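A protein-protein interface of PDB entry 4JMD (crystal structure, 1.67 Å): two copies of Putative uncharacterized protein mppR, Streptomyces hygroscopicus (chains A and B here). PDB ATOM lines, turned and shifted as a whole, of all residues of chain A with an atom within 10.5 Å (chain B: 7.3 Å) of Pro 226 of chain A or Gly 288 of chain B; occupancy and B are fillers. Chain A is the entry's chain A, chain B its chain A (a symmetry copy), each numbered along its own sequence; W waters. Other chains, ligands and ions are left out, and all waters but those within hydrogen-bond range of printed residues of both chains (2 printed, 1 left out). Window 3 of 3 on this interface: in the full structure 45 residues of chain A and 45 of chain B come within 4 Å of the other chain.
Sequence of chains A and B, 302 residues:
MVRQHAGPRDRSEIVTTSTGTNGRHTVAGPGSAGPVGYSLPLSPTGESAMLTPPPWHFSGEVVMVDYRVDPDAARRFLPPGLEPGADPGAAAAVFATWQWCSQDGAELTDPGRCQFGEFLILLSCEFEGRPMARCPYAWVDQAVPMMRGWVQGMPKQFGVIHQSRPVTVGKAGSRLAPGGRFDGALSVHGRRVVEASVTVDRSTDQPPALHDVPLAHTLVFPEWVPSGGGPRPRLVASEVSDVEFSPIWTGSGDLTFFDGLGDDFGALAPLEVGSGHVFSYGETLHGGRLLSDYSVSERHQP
The backbone NH of Gly 288 of chain B is in hydrogen-bond range of the backbone carbonyl oxygen of Trp 224 of chain A (3.0 Å).
N of Glu 239 of chain B lies within hydrogen-bond range of O of Gly 287 of chain B (3.0 Å).
Among the printed residues, pairs that only touch across the chains: Trp 224 of chain A with Gln 152 of chain B (3.6 Å), Trp 224 of chain A with Leu 285 of chain B (3.7 Å), Trp 224 of chain A with Gly 287 of chain B (3.3 Å), Val 225 of chain A with Val 236 of chain B (3.9 Å), Val 225 of chain A with Gly 288 of chain B (3.9 Å) and Pro 226 of chain A with Gly 288 of chain B (3.7 Å).
Printed residues of chain A within 4 Å of Gly 288 of chain B: Trp 224 (3.0 Å), Val 225 (3.9 Å) and Pro 226 (3.7 Å). No residue of chain A comes within 4 Å of Ala 237 of chain B. No residue of chain A comes within 4 Å of Glu 239 of chain B. Gly 287 of chain B touches just one residue of chain A: Trp 224. Printed residues of chain B within 4 Å of Val 225 of chain A: Val 236 (3.9 Å) and Gly 288 (3.9 Å). Of the printed residues of chain A, Leu 285 of chain B touches Trp 224 (3.7 Å). Arg 232 of chain A touches none of the printed residues of chain B. His 286 of chain B touches none of the printed residues of chain A. The nearest residue of chain B that does not touch Pro 226 of chain A is Gly 287 of chain B (5.7 Å). The nearest printed residue of chain A that does not touch Gln 152 of chain B is Pro 222 of chain A (6.9 Å).
Of the 6 printed residues of chain A, 3 touch a printed residue of chain B. Hydrophobic or aromatic side chains of chain A that line the printed part of chain B: Trp 224, Val 225 and Pro 226.
No position is printed for both chains.
Water W2 lies within hydrogen-bond range of NE1 of Trp 224 of chain A (2.9 Å), OG of Ser 238 of chain B (2.9 Å) and O of Gln 152 of chain B (2.9 Å). Water W1 lies within hydrogen-bond range of NH2 of Arg 234 of chain B and O of Pro 222 of chain A.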
ATOM      1  N   PRO A 222       8.796  17.048 -19.366  1.00  0.00           N
ATOM      2  CA  PRO A 222       8.365  15.934 -20.195  1.00  0.00           C
ATOM      3  C   PRO A 222       8.965  16.015 -21.593  1.00  0.00           C
ATOM      4  O   PRO A 222       9.087  17.124 -22.112  1.00  0.00           O
ATOM      5  CB  PRO A 222       6.846  16.140 -20.276  1.00  0.00           C
ATOM      6  CG  PRO A 222       6.518  16.861 -19.075  1.00  0.00           C
ATOM      7  CD  PRO A 222       7.659  17.783 -18.789  1.00  0.00           C
ATOM      8  N   GLU A 223       9.321  14.868 -22.155  1.00  0.00           N
ATOM      9  CA  GLU A 223       9.851  14.778 -23.504  1.00  0.00           C
ATOM     10  C   GLU A 223       8.692  14.706 -24.484  1.00  0.00           C
ATOM     11  O   GLU A 223       7.971  13.717 -24.544  1.00  0.00           O
ATOM     12  CB  GLU A 223      10.702  13.517 -23.690  1.00  0.00           C
ATOM     13  CG  GLU A 223      11.985  13.432 -22.855  1.00  0.00           C
ATOM     14  CD  GLU A 223      12.686  12.073 -22.996  1.00  0.00           C
ATOM     15  OE1 GLU A 223      12.266  11.271 -23.858  1.00  0.00           O
ATOM     16  OE2 GLU A 223      13.652  11.806 -22.241  1.00  0.00           O
ATOM     17  N   TRP A 224       8.573  15.745 -25.279  1.00  0.00           N
ATOM     18  CA  TRP A 224       7.514  15.868 -26.263  1.00  0.00           C
ATOM     19  C   TRP A 224       7.855  15.114 -27.552  1.00  0.00           C
ATOM     20  O   TRP A 224       7.003  14.481 -28.166  1.00  0.00           O
ATOM     21  CB  TRP A 224       7.311  17.350 -26.506  1.00  0.00           C
ATOM     22  CG  TRP A 224       6.229  17.678 -27.419  1.00  0.00           C
ATOM     23  CD1 TRP A 224       6.325  18.418 -28.563  1.00  0.00           C
ATOM     24  CD2 TRP A 224       4.849  17.305 -27.299  1.00  0.00           C
ATOM     25  NE1 TRP A 224       5.108  18.525 -29.157  1.00  0.00           N
ATOM     26  CE2 TRP A 224       4.177  17.862 -28.406  1.00  0.00           C
ATOM     27  CE3 TRP A 224       4.119  16.563 -26.366  1.00  0.00           C
ATOM     28  CZ2 TRP A 224       2.802  17.684 -28.620  1.00  0.00           C
ATOM     29  CZ3 TRP A 224       2.755  16.406 -26.565  1.00  0.00           C
ATOM     30  CH2 TRP A 224       2.114  16.966 -27.676  1.00  0.00           C
ATOM     31  N   VAL A 225       9.121  15.128 -27.947  1.00  0.00           N
ATOM     32  CA  VAL A 225       9.520  14.353 -29.112  1.00  0.00           C
ATOM     33  C   VAL A 225      10.194  13.073 -28.631  1.00  0.00           C
ATOM     34  O   VAL A 225      11.190  13.136 -27.920  1.00  0.00           O
ATOM     35  CB  VAL A 225      10.484  15.131 -30.004  1.00  0.00           C
ATOM     36  CG1 VAL A 225      10.869  14.285 -31.218  1.00  0.00           C
ATOM     37  CG2 VAL A 225       9.850  16.440 -30.438  1.00  0.00           C
ATOM     38  N   PRO A 226       9.625  11.912 -28.987  1.00  0.00           N
ATOM     39  CA  PRO A 226      10.242  10.627 -28.630  1.00  0.00           C
ATOM     40  C   PRO A 226      11.505  10.357 -29.439  1.00  0.00           C
ATOM     41  O   PRO A 226      12.545  10.873 -29.033  1.00  0.00           O
ATOM     42  CB  PRO A 226       9.153   9.603 -28.974  1.00  0.00           C
ATOM     43  CG  PRO A 226       7.880  10.383 -29.028  1.00  0.00           C
ATOM     44  CD  PRO A 226       8.269  11.737 -29.532  1.00  0.00           C
ATOM     45  N   ARG A 232      15.734  12.839 -18.925  1.00  0.00           N
ATOM     46  CA  ARG A 232      17.022  12.899 -18.230  1.00  0.00           C
ATOM     47  C   ARG A 232      17.001  13.879 -17.054  1.00  0.00           C
ATOM     48  O   ARG A 232      17.398  15.041 -17.198  1.00  0.00           O
ATOM     49  CB  ARG A 232      18.130  13.308 -19.200  1.00  0.00           C
ATOM     50  CG  ARG A 232      18.397  12.294 -20.293  1.00  0.00           C
ATOM     51  CD  ARG A 232      18.964  11.007 -19.711  1.00  0.00           C
ATOM     52  NE  ARG A 232      19.273   9.997 -20.730  1.00  0.00           N
ATOM     53  CZ  ARG A 232      18.511   8.940 -21.016  1.00  0.00           C
ATOM     54  NH1 ARG A 232      17.368   8.723 -20.372  1.00  0.00           N
ATOM     55  NH2 ARG A 232      18.896   8.089 -21.956  1.00  0.00           N
ATOM     56  N   PRO B  54       0.374  12.218 -23.105  1.00  0.00           N
ATOM     57  CA  PRO B  54      -0.534  12.224 -24.253  1.00  0.00           C
ATOM     58  C   PRO B  54      -0.869  10.778 -24.637  1.00  0.00           C
ATOM     59  O   PRO B  54      -0.167   9.862 -24.195  1.00  0.00           O
ATOM     60  CB  PRO B  54       0.279  12.916 -25.340  1.00  0.00           C
ATOM     61  CG  PRO B  54       1.723  12.688 -24.957  1.00  0.00           C
ATOM     62  CD  PRO B  54       1.739  12.647 -23.455  1.00  0.00           C
ATOM     63  N   GLN B 152       4.811  21.478 -25.356  1.00  0.00           N
ATOM     64  CA  GLN B 152       4.674  21.351 -26.812  1.00  0.00           C
ATOM     65  C   GLN B 152       5.376  22.457 -27.562  1.00  0.00           C
ATOM     66  O   GLN B 152       5.443  22.422 -28.786  1.00  0.00           O
ATOM     67  CB  GLN B 152       3.223  21.435 -27.242  1.00  0.00           C
ATOM     68  CG  GLN B 152       2.218  20.567 -26.613  1.00  0.00           C
ATOM     69  CD  GLN B 152       0.833  21.214 -26.758  1.00  0.00           C
ATOM     70  OE1 GLN B 152       0.394  21.568 -27.859  1.00  0.00           O
ATOM     71  NE2 GLN B 152       0.173  21.426 -25.642  1.00  0.00           N
ATOM     72  N   LEU B 219      10.360  24.467 -29.180  1.00  0.00           N
ATOM     73  CA  LEU B 219      10.518  23.839 -27.880  1.00  0.00           C
ATOM     74  C   LEU B 219      11.808  24.319 -27.253  1.00  0.00           C
ATOM     75  O   LEU B 219      12.895  23.968 -27.715  1.00  0.00           O
ATOM     76  CB  LEU B 219      10.533  22.316 -28.077  1.00  0.00           C
ATOM     77  CG  LEU B 219      10.560  21.401 -26.864  1.00  0.00           C
ATOM     78  CD1 LEU B 219       9.420  21.750 -25.948  1.00  0.00           C
ATOM     79  CD2 LEU B 219      10.454  19.954 -27.332  1.00  0.00           C
ATOM     80  N   ARG B 234      14.435  23.502 -30.349  1.00  0.00           N
ATOM     81  CA  ARG B 234      14.071  22.589 -31.431  1.00  0.00           C
ATOM     82  C   ARG B 234      12.773  23.060 -32.060  1.00  0.00           C
ATOM     83  O   ARG B 234      11.856  23.493 -31.367  1.00  0.00           O
ATOM     84  CB  ARG B 234      13.900  21.163 -30.912  1.00  0.00           C
ATOM     85  CG  ARG B 234      15.197  20.506 -30.466  1.00  0.00           C
ATOM     86  CD  ARG B 234      14.889  19.163 -29.808  1.00  0.00           C
ATOM     87  NE  ARG B 234      14.328  19.326 -28.466  1.00  0.00           N
ATOM     88  CZ  ARG B 234      13.737  18.353 -27.775  1.00  0.00           C
ATOM     89  NH1 ARG B 234      13.633  17.135 -28.291  1.00  0.00           N
ATOM     90  NH2 ARG B 234      13.255  18.597 -26.563  1.00  0.00           N
ATOM     91  N   VAL B 236       9.463  22.050 -33.725  1.00  0.00           N
ATOM     92  CA  VAL B 236       8.636  20.857 -33.708  1.00  0.00           C
ATOM     93  C   VAL B 236       7.232  21.129 -34.223  1.00  0.00           C
ATOM     94  O   VAL B 236       6.769  22.264 -34.250  1.00  0.00           O
ATOM     95  CB  VAL B 236       8.555  20.277 -32.312  1.00  0.00           C
ATOM     96  CG1 VAL B 236       9.963  20.065 -31.759  1.00  0.00           C
ATOM     97  CG2 VAL B 236       7.769  21.204 -31.392  1.00  0.00           C
ATOM     98  N   ALA B 237       6.587  20.063 -34.678  1.00  0.00           N
ATOM     99  CA  ALA B 237       5.195  20.133 -35.113  1.00  0.00           C
ATOM    100  C   ALA B 237       4.371  19.266 -34.183  1.00  0.00           C
ATOM    101  O   ALA B 237       4.818  18.227 -33.687  1.00  0.00           O
ATOM    102  CB  ALA B 237       5.054  19.665 -36.550  1.00  0.00           C
ATOM    103  N   SER B 238       3.148  19.700 -33.927  1.00  0.00           N
ATOM    104  CA  SER B 238       2.238  18.904 -33.169  1.00  0.00           C
ATOM    105  C   SER B 238       1.614  17.871 -34.077  1.00  0.00           C
ATOM    106  O   SER B 238       0.972  18.220 -35.079  1.00  0.00           O
ATOM    107  CB  SER B 238       1.137  19.802 -32.569  1.00  0.00           C
ATOM    108  OG  SER B 238       1.651  20.652 -31.542  1.00  0.00           O
ATOM    109  N   GLU B 239       1.829  16.603 -33.740  1.00  0.00           N
ATOM    110  CA  GLU B 239       1.156  15.482 -34.384  1.00  0.00           C
ATOM    111  C   GLU B 239      -0.276  15.246 -33.894  1.00  0.00           C
ATOM    112  O   GLU B 239      -0.496  14.881 -32.731  1.00  0.00           O
ATOM    113  CB  GLU B 239       1.930  14.200 -34.151  1.00  0.00           C
ATOM    114  CG  GLU B 239       3.285  14.202 -34.817  1.00  0.00           C
ATOM    115  CD  GLU B 239       3.648  12.842 -35.374  1.00  0.00           C
ATOM    116  OE1 GLU B 239       3.985  11.938 -34.578  1.00  0.00           O
ATOM    117  OE2 GLU B 239       3.574  12.676 -36.608  1.00  0.00           O
ATOM    118  N   LEU B 285      -4.259  15.207 -29.821  1.00  0.00           N
ATOM    119  CA  LEU B 285      -2.845  15.587 -29.854  1.00  0.00           C
ATOM    120  C   LEU B 285      -2.011  14.449 -29.290  1.00  0.00           C
ATOM    121  O   LEU B 285      -2.227  14.016 -28.167  1.00  0.00           O
ATOM    122  CB  LEU B 285      -2.661  16.863 -29.031  1.00  0.00           C
ATOM    123  CG  LEU B 285      -1.338  17.602 -28.984  1.00  0.00           C
ATOM    124  CD1 LEU B 285      -0.870  18.040 -30.364  1.00  0.00           C
ATOM    125  CD2 LEU B 285      -1.514  18.816 -28.064  1.00  0.00           C
ATOM    126  N   HIS B 286      -1.084  13.925 -30.089  1.00  0.00           N
ATOM    127  CA  HIS B 286      -0.371  12.702 -29.705  1.00  0.00           C
ATOM    128  C   HIS B 286       1.042  12.928 -29.158  1.00  0.00           C
ATOM    129  O   HIS B 286       1.559  12.084 -28.421  1.00  0.00           O
ATOM    130  CB  HIS B 286      -0.256  11.739 -30.901  1.00  0.00           C
ATOM    131  CG  HIS B 286      -1.565  11.187 -31.344  1.00  0.00           C
ATOM    132  ND1 HIS B 286      -2.086  10.015 -30.843  1.00  0.00           N
ATOM    133  CD2 HIS B 286      -2.490  11.674 -32.202  1.00  0.00           C
ATOM    134  CE1 HIS B 286      -3.265   9.792 -31.390  1.00  0.00           C
ATOM    135  NE2 HIS B 286      -3.534  10.786 -32.216  1.00  0.00           N
ATOM    136  N   GLY B 287       1.671  14.020 -29.545  1.00  0.00           N
ATOM    137  CA  GLY B 287       3.094  14.164 -29.307  1.00  0.00           C
ATOM    138  C   GLY B 287       3.713  15.067 -30.335  1.00  0.00           C
ATOM    139  O   GLY B 287       3.020  15.633 -31.192  1.00  0.00           O
ATOM    140  N   GLY B 288       5.028  15.239 -30.245  1.00  0.00           N
ATOM    141  CA  GLY B 288       5.712  16.100 -31.171  1.00  0.00           C
ATOM    142  C   GLY B 288       6.470  15.304 -32.221  1.00  0.00           C
ATOM    143  O   GLY B 288       6.856  14.156 -31.986  1.00  0.00           O
ATOM    144  N   ARG B 289       6.642  15.910 -33.382  1.00  0.00           N
ATOM    145  CA  ARG B 289       7.579  15.385 -34.369  1.00  0.00           C
ATOM    146  C   ARG B 289       8.606  16.464 -34.636  1.00  0.00           C
ATOM    147  O   ARG B 289       8.285  17.653 -34.725  1.00  0.00           O
ATOM    148  CB  ARG B 289       6.872  14.983 -35.643  1.00  0.00           C
ATOM    149  CG  ARG B 289       6.075  16.065 -36.295  1.00  0.00           C
ATOM    150  CD  ARG B 289       5.189  15.473 -37.380  1.00  0.00           C
ATOM    151  NE  ARG B 289       4.219  16.440 -37.887  1.00  0.00           N
ATOM    152  CZ  ARG B 289       4.392  17.163 -38.988  1.00  0.00           C
ATOM    153  NH1 ARG B 289       5.495  17.037 -39.720  1.00  0.00           N
ATOM    154  NH2 ARG B 289       3.451  18.016 -39.367  1.00  0.00           N
ATOM    155  N   LEU B 290       9.854  16.051 -34.744  1.00  0.00           N
ATOM    156  CA  LEU B 290      10.922  17.010 -34.931  1.00  0.00           C
ATOM    157  C   LEU B 290      10.935  17.535 -36.352  1.00  0.00           C
ATOM    158  O   LEU B 290      10.962  16.761 -37.316  1.00  0.00           O
ATOM    159  CB  LEU B 290      12.264  16.365 -34.603  1.00  0.00           C
ATOM    160  CG  LEU B 290      13.489  17.265 -34.715  1.00  0.00           C
ATOM    161  CD1 LEU B 290      13.465  18.350 -33.659  1.00  0.00           C
ATOM    162  CD2 LEU B 290      14.771  16.446 -34.576  1.00  0.00           C
ATOM    163  N   LEU B 291      10.923  18.857 -36.488  1.00  0.00           N
ATOM    164  CA  LEU B 291      11.137  19.474 -37.792  1.00  0.00           C
ATOM    165  C   LEU B 291      12.620  19.782 -37.976  1.00  0.00           C
ATOM    166  O   LEU B 291      13.205  19.476 -39.023  1.00  0.00           O
ATOM    167  CB  LEU B 291      10.297  20.751 -37.939  1.00  0.00           C
ATOM    168  CG  LEU B 291       8.785  20.574 -37.839  1.00  0.00           C
ATOM    169  CD1 LEU B 291       8.085  21.882 -38.131  1.00  0.00           C
ATOM    170  CD2 LEU B 291       8.303  19.475 -38.775  1.00  0.00           C
HETATM  171  O   HOH W   1      11.294  18.508 -24.248  1.00  0.00           O
HETATM  172  O   HOH W   2       4.431  20.699 -30.876  1.00  0.00           O
